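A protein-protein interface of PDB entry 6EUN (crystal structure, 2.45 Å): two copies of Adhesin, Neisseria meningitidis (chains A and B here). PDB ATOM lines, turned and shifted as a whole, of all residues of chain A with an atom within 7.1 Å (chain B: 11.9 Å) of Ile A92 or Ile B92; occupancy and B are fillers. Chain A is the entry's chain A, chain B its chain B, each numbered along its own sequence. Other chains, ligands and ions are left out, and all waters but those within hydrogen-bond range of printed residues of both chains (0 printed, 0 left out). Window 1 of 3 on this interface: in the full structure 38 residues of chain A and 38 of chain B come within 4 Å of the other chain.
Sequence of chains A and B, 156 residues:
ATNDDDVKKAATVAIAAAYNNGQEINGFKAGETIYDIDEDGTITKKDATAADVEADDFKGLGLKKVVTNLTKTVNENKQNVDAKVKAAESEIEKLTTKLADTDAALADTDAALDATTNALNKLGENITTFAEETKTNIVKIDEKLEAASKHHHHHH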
ATOM      1  N   VAL A  85     -15.943  18.749  -4.430  1.00  0.00           N
ATOM      2  CA  VAL A  85     -15.506  18.407  -5.790  1.00  0.00           C
ATOM      3  C   VAL A  85     -16.194  19.337  -6.817  1.00  0.00           C
ATOM      4  O   VAL A  85     -15.537  19.760  -7.772  1.00  0.00           O
ATOM      5  CB  VAL A  85     -15.654  16.881  -6.099  1.00  0.00           C
ATOM      6  CG1 VAL A  85     -15.494  16.570  -7.582  1.00  0.00           C
ATOM      7  CG2 VAL A  85     -14.662  16.059  -5.280  1.00  0.00           C
ATOM      8  N   ALA A  87     -17.122  22.400  -6.175  1.00  0.00           N
ATOM      9  CA  ALA A  87     -16.481  23.690  -5.918  1.00  0.00           C
ATOM     10  C   ALA A  87     -15.143  23.763  -6.673  1.00  0.00           C
ATOM     11  O   ALA A  87     -14.933  24.705  -7.436  1.00  0.00           O
ATOM     12  CB  ALA A  87     -16.269  23.891  -4.423  1.00  0.00           C
ATOM     13  N   ALA A  88     -14.280  22.738  -6.505  1.00  0.00           N
ATOM     14  CA  ALA A  88     -12.973  22.616  -7.159  1.00  0.00           C
ATOM     15  C   ALA A  88     -13.099  22.643  -8.689  1.00  0.00           C
ATOM     16  O   ALA A  88     -12.311  23.315  -9.346  1.00  0.00           O
ATOM     17  CB  ALA A  88     -12.276  21.338  -6.708  1.00  0.00           C
ATOM     18  N   GLU A  89     -14.106  21.945  -9.238  1.00  0.00           N
ATOM     19  CA  GLU A  89     -14.374  21.891 -10.672  1.00  0.00           C
ATOM     20  C   GLU A  89     -14.805  23.247 -11.239  1.00  0.00           C
ATOM     21  O   GLU A  89     -14.520  23.533 -12.408  1.00  0.00           O
ATOM     22  CB  GLU A  89     -15.437  20.825 -10.984  1.00  0.00           C
ATOM     23  CG  GLU A  89     -14.879  19.422 -11.143  1.00  0.00           C
ATOM     24  CD  GLU A  89     -14.010  19.219 -12.372  1.00  0.00           C
ATOM     25  OE1 GLU A  89     -14.571  19.074 -13.484  1.00  0.00           O
ATOM     26  OE2 GLU A  89     -12.767  19.224 -12.223  1.00  0.00           O
ATOM     27  N   SER A  90     -15.510  24.068 -10.427  1.00  0.00           N
ATOM     28  CA  SER A  90     -15.954  25.402 -10.824  1.00  0.00           C
ATOM     29  C   SER A  90     -14.760  26.347 -10.868  1.00  0.00           C
ATOM     30  O   SER A  90     -14.698  27.204 -11.747  1.00  0.00           O
ATOM     31  CB  SER A  90     -17.025  25.924  -9.874  1.00  0.00           C
ATOM     32  OG  SER A  90     -18.306  25.471 -10.278  1.00  0.00           O
ATOM     33  N   GLU A  91     -13.800  26.162  -9.942  1.00  0.00           N
ATOM     34  CA  GLU A  91     -12.562  26.926  -9.870  1.00  0.00           C
ATOM     35  C   GLU A  91     -11.714  26.593 -11.096  1.00  0.00           C
ATOM     36  O   GLU A  91     -11.179  27.504 -11.729  1.00  0.00           O
ATOM     37  CB  GLU A  91     -11.808  26.623  -8.572  1.00  0.00           C
ATOM     38  CG  GLU A  91     -12.372  27.354  -7.359  1.00  0.00           C
ATOM     39  CD  GLU A  91     -12.089  26.737  -5.998  1.00  0.00           C
ATOM     40  OE1 GLU A  91     -10.897  26.547  -5.661  1.00  0.00           O
ATOM     41  OE2 GLU A  91     -13.060  26.489  -5.246  1.00  0.00           O
ATOM     42  N   ILE A  92     -11.655  25.299 -11.467  1.00  0.00           N
ATOM     43  CA  ILE A  92     -10.951  24.792 -12.647  1.00  0.00           C
ATOM     44  C   ILE A  92     -11.575  25.403 -13.916  1.00  0.00           C
ATOM     45  O   ILE A  92     -10.837  25.857 -14.796  1.00  0.00           O
ATOM     46  CB  ILE A  92     -10.906  23.231 -12.655  1.00  0.00           C
ATOM     47  CG1 ILE A  92      -9.907  22.711 -11.608  1.00  0.00           C
ATOM     48  CG2 ILE A  92     -10.586  22.652 -14.043  1.00  0.00           C
ATOM     49  CD1 ILE A  92     -10.152  21.239 -11.137  1.00  0.00           C
ATOM     50  N   GLU A  93     -12.915  25.454 -13.987  1.00  0.00           N
ATOM     51  CA  GLU A  93     -13.626  26.012 -15.141  1.00  0.00           C
ATOM     52  C   GLU A  93     -13.303  27.508 -15.323  1.00  0.00           C
ATOM     53  O   GLU A  93     -13.095  27.951 -16.454  1.00  0.00           O
ATOM     54  CB  GLU A  93     -15.142  25.745 -15.029  1.00  0.00           C
ATOM     55  CG  GLU A  93     -15.930  25.884 -16.327  1.00  0.00           C
ATOM     56  CD  GLU A  93     -16.201  27.312 -16.763  1.00  0.00           C
ATOM     57  OE1 GLU A  93     -15.771  27.683 -17.878  1.00  0.00           O
ATOM     58  OE2 GLU A  93     -16.763  28.087 -15.954  1.00  0.00           O
ATOM     59  N   LYS A  94     -13.236  28.262 -14.212  1.00  0.00           N
ATOM     60  CA  LYS A  94     -12.929  29.690 -14.226  1.00  0.00           C
ATOM     61  C   LYS A  94     -11.457  29.983 -14.591  1.00  0.00           C
ATOM     62  O   LYS A  94     -11.181  30.990 -15.243  1.00  0.00           O
ATOM     63  CB  LYS A  94     -13.349  30.358 -12.911  1.00  0.00           C
ATOM     64  CG  LYS A  94     -14.868  30.500 -12.808  1.00  0.00           C
ATOM     65  CD  LYS A  94     -15.333  31.254 -11.565  1.00  0.00           C
ATOM     66  CE  LYS A  94     -16.841  31.328 -11.475  1.00  0.00           C
ATOM     67  NZ  LYS A  94     -17.416  32.273 -12.473  1.00  0.00           N
ATOM     68  N   LEU A  95     -10.529  29.089 -14.201  1.00  0.00           N
ATOM     69  CA  LEU A  95      -9.103  29.196 -14.518  1.00  0.00           C
ATOM     70  C   LEU A  95      -8.885  28.926 -16.003  1.00  0.00           C
ATOM     71  O   LEU A  95      -7.986  29.512 -16.597  1.00  0.00           O
ATOM     72  CB  LEU A  95      -8.268  28.196 -13.702  1.00  0.00           C
ATOM     73  CG  LEU A  95      -7.792  28.637 -12.328  1.00  0.00           C
ATOM     74  CD1 LEU A  95      -7.314  27.427 -11.511  1.00  0.00           C
ATOM     75  CD2 LEU A  95      -6.669  29.664 -12.429  1.00  0.00           C
ATOM     76  N   THR A  96      -9.692  28.019 -16.586  1.00  0.00           N
ATOM     77  CA  THR A  96      -9.652  27.628 -17.998  1.00  0.00           C
ATOM     78  C   THR A  96     -10.076  28.812 -18.882  1.00  0.00           C
ATOM     79  O   THR A  96      -9.407  29.112 -19.870  1.00  0.00           O
ATOM     80  CB  THR A  96     -10.521  26.366 -18.216  1.00  0.00           C
ATOM     81  OG1 THR A  96      -9.980  25.280 -17.456  1.00  0.00           O
ATOM     82  CG2 THR A  96     -10.634  25.962 -19.687  1.00  0.00           C
ATOM     83  N   THR A  97     -11.179  29.479 -18.518  1.00  0.00           N
ATOM     84  CA  THR A  97     -11.698  30.603 -19.284  1.00  0.00           C
ATOM     85  C   THR A  97     -10.722  31.801 -19.199  1.00  0.00           C
ATOM     86  O   THR A  97     -10.471  32.433 -20.222  1.00  0.00           O
ATOM     87  CB  THR A  97     -13.171  30.901 -18.916  1.00  0.00           C
ATOM     88  OG1 THR A  97     -13.750  31.736 -19.918  1.00  0.00           O
ATOM     89  CG2 THR A  97     -13.343  31.542 -17.548  1.00  0.00           C
ATOM     90  N   LYS A  98     -10.127  32.050 -18.015  1.00  0.00           N
ATOM     91  CA  LYS A  98      -9.185  33.141 -17.799  1.00  0.00           C
ATOM     92  C   LYS A  98      -7.880  32.890 -18.565  1.00  0.00           C
ATOM     93  O   LYS A  98      -7.365  33.826 -19.182  1.00  0.00           O
ATOM     94  CB  LYS A  98      -8.938  33.390 -16.297  1.00  0.00           C
ATOM     95  CG  LYS A  98      -8.090  34.634 -15.970  1.00  0.00           C
ATOM     96  CD  LYS A  98      -8.887  35.933 -15.919  1.00  0.00           C
ATOM     97  CE  LYS A  98      -8.366  36.952 -16.905  1.00  0.00           C
ATOM     98  NZ  LYS A  98      -9.056  38.261 -16.762  1.00  0.00           N
ATOM     99  N   VAL B  81     -15.929   8.782  -6.369  1.00  0.00           N
ATOM    100  CA  VAL B  81     -15.208   9.992  -5.984  1.00  0.00           C
ATOM    101  C   VAL B  81     -13.729   9.913  -6.415  1.00  0.00           C
ATOM    102  O   VAL B  81     -13.182  10.931  -6.830  1.00  0.00           O
ATOM    103  CB  VAL B  81     -15.405  10.382  -4.495  1.00  0.00           C
ATOM    104  CG1 VAL B  81     -14.589   9.505  -3.548  1.00  0.00           C
ATOM    105  CG2 VAL B  81     -15.109  11.857  -4.269  1.00  0.00           C
ATOM    106  N   ASP B  82     -13.112   8.714  -6.370  1.00  0.00           N
ATOM    107  CA  ASP B  82     -11.718   8.512  -6.781  1.00  0.00           C
ATOM    108  C   ASP B  82     -11.505   8.917  -8.253  1.00  0.00           C
ATOM    109  O   ASP B  82     -10.463   9.484  -8.580  1.00  0.00           O
ATOM    110  CB  ASP B  82     -11.272   7.048  -6.558  1.00  0.00           C
ATOM    111  CG  ASP B  82     -10.747   6.687  -5.172  1.00  0.00           C
ATOM    112  OD1 ASP B  82     -10.801   7.552  -4.263  1.00  0.00           O
ATOM    113  OD2 ASP B  82     -10.283   5.537  -4.995  1.00  0.00           O
ATOM    114  N   ALA B  83     -12.507   8.638  -9.113  1.00  0.00           N
ATOM    115  CA  ALA B  83     -12.524   8.934 -10.541  1.00  0.00           C
ATOM    116  C   ALA B  83     -12.828  10.405 -10.823  1.00  0.00           C
ATOM    117  O   ALA B  83     -12.326  10.941 -11.809  1.00  0.00           O
ATOM    118  CB  ALA B  83     -13.529   8.046 -11.248  1.00  0.00           C
ATOM    119  N   LYS B  84     -13.649  11.057  -9.975  1.00  0.00           N
ATOM    120  CA  LYS B  84     -13.975  12.481 -10.103  1.00  0.00           C
ATOM    121  C   LYS B  84     -12.725  13.290  -9.752  1.00  0.00           C
ATOM    122  O   LYS B  84     -12.387  14.237 -10.462  1.00  0.00           O
ATOM    123  CB  LYS B  84     -15.147  12.869  -9.188  1.00  0.00           C
ATOM    124  CG  LYS B  84     -16.517  12.503  -9.748  1.00  0.00           C
ATOM    125  CD  LYS B  84     -17.633  12.798  -8.743  1.00  0.00           C
ATOM    126  CE  LYS B  84     -18.999  12.417  -9.259  1.00  0.00           C
ATOM    127  NZ  LYS B  84     -20.050  12.621  -8.226  1.00  0.00           N
ATOM    128  N   VAL B  85     -12.014  12.870  -8.688  1.00  0.00           N
ATOM    129  CA  VAL B  85     -10.763  13.479  -8.214  1.00  0.00           C
ATOM    130  C   VAL B  85      -9.629  13.241  -9.247  1.00  0.00           C
ATOM    131  O   VAL B  85      -8.828  14.148  -9.476  1.00  0.00           O
ATOM    132  CB  VAL B  85     -10.408  13.039  -6.753  1.00  0.00           C
ATOM    133  CG1 VAL B  85      -8.983  13.423  -6.369  1.00  0.00           C
ATOM    134  CG2 VAL B  85     -11.395  13.623  -5.749  1.00  0.00           C
ATOM    135  N   LYS B  86      -9.602  12.061  -9.902  1.00  0.00           N
ATOM    136  CA  LYS B  86      -8.599  11.750 -10.926  1.00  0.00           C
ATOM    137  C   LYS B  86      -8.831  12.613 -12.170  1.00  0.00           C
ATOM    138  O   LYS B  86      -7.863  13.003 -12.830  1.00  0.00           O
ATOM    139  CB  LYS B  86      -8.593  10.260 -11.292  1.00  0.00           C
ATOM    140  CG  LYS B  86      -7.272   9.796 -11.889  1.00  0.00           C
ATOM    141  CD  LYS B  86      -7.363   8.368 -12.393  1.00  0.00           C
ATOM    142  CE  LYS B  86      -6.011   7.796 -12.738  1.00  0.00           C
ATOM    143  NZ  LYS B  86      -6.107   6.359 -13.117  1.00  0.00           N
ATOM    144  N   ALA B  87     -10.115  12.929 -12.462  1.00  0.00           N
ATOM    145  CA  ALA B  87     -10.521  13.780 -13.582  1.00  0.00           C
ATOM    146  C   ALA B  87     -10.059  15.215 -13.325  1.00  0.00           C
ATOM    147  O   ALA B  87      -9.373  15.784 -14.174  1.00  0.00           O
ATOM    148  CB  ALA B  87     -12.033  13.730 -13.771  1.00  0.00           C
ATOM    149  N   ALA B  88     -10.381  15.768 -12.133  1.00  0.00           N
ATOM    150  CA  ALA B  88     -10.008  17.118 -11.699  1.00  0.00           C
ATOM    151  C   ALA B  88      -8.489  17.311 -11.709  1.00  0.00           C
ATOM    152  O   ALA B  88      -8.021  18.349 -12.164  1.00  0.00           O
ATOM    153  CB  ALA B  88     -10.568  17.404 -10.312  1.00  0.00           C
ATOM    154  N   GLU B  89      -7.731  16.305 -11.246  1.00  0.00           N
ATOM    155  CA  GLU B  89      -6.269  16.327 -11.215  1.00  0.00           C
ATOM    156  C   GLU B  89      -5.655  16.355 -12.619  1.00  0.00           C
ATOM    157  O   GLU B  89      -4.583  16.937 -12.794  1.00  0.00           O
ATOM    158  CB  GLU B  89      -5.722  15.131 -10.417  1.00  0.00           C
ATOM    159  CG  GLU B  89      -5.656  15.370  -8.919  1.00  0.00           C
ATOM    160  CD  GLU B  89      -4.629  16.400  -8.483  1.00  0.00           C
ATOM    161  OE1 GLU B  89      -3.423  16.061  -8.439  1.00  0.00           O
ATOM    162  OE2 GLU B  89      -5.030  17.554  -8.205  1.00  0.00           O
ATOM    163  N   SER B  90      -6.317  15.708 -13.604  1.00  0.00           N
ATOM    164  CA  SER B  90      -5.867  15.676 -14.995  1.00  0.00           C
ATOM    165  C   SER B  90      -6.093  17.038 -15.644  1.00  0.00           C
ATOM    166  O   SER B  90      -5.265  17.481 -16.441  1.00  0.00           O
ATOM    167  CB  SER B  90      -6.580  14.578 -15.774  1.00  0.00           C
ATOM    168  OG  SER B  90      -5.906  13.341 -15.608  1.00  0.00           O
ATOM    169  N   GLU B  91      -7.195  17.716 -15.261  1.00  0.00           N
ATOM    170  CA  GLU B  91      -7.538  19.058 -15.712  1.00  0.00           C
ATOM    171  C   GLU B  91      -6.506  20.038 -15.149  1.00  0.00           C
ATOM    172  O   GLU B  91      -6.016  20.892 -15.886  1.00  0.00           O
ATOM    173  CB  GLU B  91      -8.958  19.434 -15.274  1.00  0.00           C
ATOM    174  CG  GLU B  91     -10.039  18.825 -16.160  1.00  0.00           C
ATOM    175  CD  GLU B  91     -11.419  18.674 -15.540  1.00  0.00           C
ATOM    176  OE1 GLU B  91     -11.994  19.694 -15.090  1.00  0.00           O
ATOM    177  OE2 GLU B  91     -11.949  17.539 -15.554  1.00  0.00           O
ATOM    178  N   ILE B  92      -6.132  19.868 -13.868  1.00  0.00           N
ATOM    179  CA  ILE B  92      -5.113  20.659 -13.180  1.00  0.00           C
ATOM    180  C   ILE B  92      -3.755  20.468 -13.880  1.00  0.00           C
ATOM    181  O   ILE B  92      -3.057  21.454 -14.119  1.00  0.00           O
ATOM    182  CB  ILE B  92      -5.082  20.342 -11.649  1.00  0.00           C
ATOM    183  CG1 ILE B  92      -6.301  20.959 -10.941  1.00  0.00           C
ATOM    184  CG2 ILE B  92      -3.778  20.801 -10.972  1.00  0.00           C
ATOM    185  CD1 ILE B  92      -6.677  20.280  -9.579  1.00  0.00           C
ATOM    186  N   GLU B  93      -3.410  19.224 -14.244  1.00  0.00           N
ATOM    187  CA  GLU B  93      -2.146  18.924 -14.917  1.00  0.00           C
ATOM    188  C   GLU B  93      -2.057  19.619 -16.293  1.00  0.00           C
ATOM    189  O   GLU B  93      -1.012  20.174 -16.637  1.00  0.00           O
ATOM    190  CB  GLU B  93      -1.932  17.403 -15.040  1.00  0.00           C
ATOM    191  CG  GLU B  93      -0.509  16.888 -15.291  1.00  0.00           C
ATOM    192  CD  GLU B  93       0.657  17.705 -15.841  1.00  0.00           C
ATOM    193  OE1 GLU B  93       0.820  17.779 -17.083  1.00  0.00           O
ATOM    194  OE2 GLU B  93       1.492  18.151 -15.020  1.00  0.00           O
ATOM    195  N   LYS B  94      -3.169  19.632 -17.041  1.00  0.00           N
ATOM    196  CA  LYS B  94      -3.253  20.270 -18.352  1.00  0.00           C
ATOM    197  C   LYS B  94      -3.213  21.810 -18.266  1.00  0.00           C
ATOM    198  O   LYS B  94      -2.653  22.450 -19.158  1.00  0.00           O
ATOM    199  CB  LYS B  94      -4.467  19.757 -19.142  1.00  0.00           C
ATOM    200  CG  LYS B  94      -4.258  18.333 -19.642  1.00  0.00           C
ATOM    201  CD  LYS B  94      -5.386  17.810 -20.520  1.00  0.00           C
ATOM    202  CE  LYS B  94      -5.082  16.418 -21.026  1.00  0.00           C
ATOM    203  NZ  LYS B  94      -4.073  16.433 -22.131  1.00  0.00           N
ATOM    204  N   LEU B  95      -3.777  22.399 -17.186  1.00  0.00           N
ATOM    205  CA  LEU B  95      -3.765  23.839 -16.948  1.00  0.00           C
ATOM    206  C   LEU B  95      -2.358  24.292 -16.589  1.00  0.00           C
ATOM    207  O   LEU B  95      -1.980  25.403 -16.927  1.00  0.00           O
ATOM    208  CB  LEU B  95      -4.723  24.227 -15.813  1.00  0.00           C
ATOM    209  CG  LEU B  95      -6.179  24.492 -16.188  1.00  0.00           C
ATOM    210  CD1 LEU B  95      -7.069  24.480 -14.943  1.00  0.00           C
ATOM    211  CD2 LEU B  95      -6.337  25.821 -16.929  1.00  0.00           C
ATOM    212  N   THR B  96      -1.602  23.440 -15.879  1.00  0.00           N
ATOM    213  CA  THR B  96      -0.220  23.680 -15.450  1.00  0.00           C
ATOM    214  C   THR B  96       0.708  23.741 -16.681  1.00  0.00           C
ATOM    215  O   THR B  96       1.527  24.655 -16.781  1.00  0.00           O
ATOM    216  CB  THR B  96       0.208  22.584 -14.433  1.00  0.00           C
ATOM    217  OG1 THR B  96      -0.614  22.680 -13.267  1.00  0.00           O
ATOM    218  CG2 THR B  96       1.681  22.679 -14.028  1.00  0.00           C
ATOM    219  N   THR B  97       0.574  22.772 -17.603  1.00  0.00           N
ATOM    220  CA  THR B  97       1.407  22.711 -18.791  1.00  0.00           C
ATOM    221  C   THR B  97       1.092  23.904 -19.731  1.00  0.00           C
ATOM    222  O   THR B  97       2.024  24.510 -20.256  1.00  0.00           O
ATOM    223  CB  THR B  97       1.354  21.308 -19.442  1.00  0.00           C
ATOM    224  OG1 THR B  97       2.431  21.174 -20.365  1.00  0.00           O
ATOM    225  CG2 THR B  97       0.043  21.003 -20.140  1.00  0.00           C
ATOM    226  N   LYS B  98      -0.197  24.279 -19.864  1.00  0.00           N
ATOM    227  CA  LYS B  98      -0.637  25.390 -20.701  1.00  0.00           C
ATOM    228  C   LYS B  98      -0.162  26.719 -20.124  1.00  0.00           C
ATOM    229  O   LYS B  98       0.312  27.562 -20.892  1.00  0.00           O
ATOM    230  CB  LYS B  98      -2.166  25.368 -20.923  1.00  0.00           C
ATOM    231  CG  LYS B  98      -2.701  26.399 -21.935  1.00  0.00           C
ATOM    232  CD  LYS B  98      -2.614  25.941 -23.390  1.00  0.00           C
ATOM    233  CE  LYS B  98      -1.781  26.877 -24.231  1.00  0.00           C
ATOM    234  NZ  LYS B  98      -1.795  26.477 -25.667  1.00  0.00           N
ATOM    235  N   LEU B  99      -0.244  26.896 -18.783  1.00  0.00           N
ATOM    236  CA  LEU B  99       0.220  28.115 -18.117  1.00  0.00           C
ATOM    237  C   LEU B  99       1.739  28.269 -18.253  1.00  0.00           C
ATOM    238  O   LEU B  99       2.221  29.388 -18.407  1.00  0.00           O
ATOM    239  CB  LEU B  99      -0.226  28.186 -16.644  1.00  0.00           C
ATOM    240  CG  LEU B  99       0.049  29.480 -15.860  1.00  0.00           C
ATOM    241  CD1 LEU B  99      -0.472  30.716 -16.597  1.00  0.00           C
ATOM    242  CD2 LEU B  99      -0.608  29.444 -14.514  1.00  0.00           C
ATOM    243  N   ALA B 100       2.477  27.149 -18.250  1.00  0.00           N
ATOM    244  CA  ALA B 100       3.931  27.136 -18.421  1.00  0.00           C
ATOM    245  C   ALA B 100       4.314  27.555 -19.857  1.00  0.00           C
ATOM    246  O   ALA B 100       5.328  28.233 -20.049  1.00  0.00           O
ATOM    247  CB  ALA B 100       4.484  25.758 -18.096  1.00  0.00           C
ATOM    248  N   ASP B 101       3.487  27.160 -20.849  1.00  0.00           N
ATOM    249  CA  ASP B 101       3.657  27.482 -22.262  1.00  0.00           C
ATOM    250  C   ASP B 101       3.331  28.960 -22.509  1.00  0.00           C
ATOM    251  O   ASP B 101       3.929  29.575 -23.394  1.00  0.00           O
ATOM    252  CB  ASP B 101       2.748  26.592 -23.131  1.00  0.00           C
ATOM    253  CG  ASP B 101       3.119  25.112 -23.208  1.00  0.00           C
ATOM    254  OD1 ASP B 101       4.216  24.740 -22.716  1.00  0.00           O
ATOM    255  OD2 ASP B 101       2.310  24.322 -23.766  1.00  0.00           O
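Glu A89 touches Glu B91, but with the chains exchanged Glu A91 does not touch Glu B89 (11.0 Å).
Ile A92 touches Ala B88, but with the chains exchanged Ala A88 does not touch Ile B92 (6.4 Å).
Ile A92 touches Glu B91, but with the chains exchanged Glu A91 does not touch Ile B92 (7.8 Å).
Thr A96 touches Leu B95, but with the chains exchanged Leu A95 does not touch Thr B96 (8.2 Å).
Positions printed for both chains: 85, 87, 88, 89, 90, 91, 92, 93, 94, 95, 96, 97 and 98.
Of the 6 pairs that touch across the chains among the printed residues, 1 has its exchanged pair printed and touching as well.
Among the printed residues, pairs that only touch across the chains: Glu A89 with Ala B88, Ile A92 with Glu B91, Thr A96 with Leu B95, Ile A92 with Ala B88 and Ile A92 with Ile B92.
Among the printed residues, no Asp or Glu carboxylate lies within 4 Å of a Lys or Arg side-chain nitrogen of the other chain.
No residue of chain B comes within 4 Å of Ser A90.
No residue of chain B comes within 4 Å of Glu A93.
No residue of chain B comes within 4 Å of Leu A95.
Thr A96 touches just one residue of chain B: Leu B95.
Printed residues of chain A within 4 Å of Glu B91: Glu A89 and Ile A92.
Printed residues of chain A within 4 Å of Ala B88: Glu A89 and Ile A92.
Of the printed residues of chain A, Leu B95 touches Thr A96 (3.7 Å).
Lys B98 touches none of the printed residues of chain A.
The nearest printed residue of chain B that does not touch Ile A92 is Leu B95 (4.01 Å).
The nearest residue of chain A that does not touch Ile B92 is Ala A88 (6.4 Å).
The nearest printed residue of chain A that does not touch Leu B95 is Ile A92 (4.01 Å).
The side-chain carboxylate (OE1) of Glu B91 lies close to the side-chain carboxylate (OE2) of Glu A89, 3.0 Å away.
The side-chain hydroxyl of Thr B96 sits at hydrogen-bond distance from the backbone carbonyl oxygen of Ile B92 (2.9 Å).
The side-chain hydroxyl (OG1) of Thr A96 is in hydrogen-bond range of the backbone carbonyl oxygen (O) of Ile A92 (2.9 Å).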
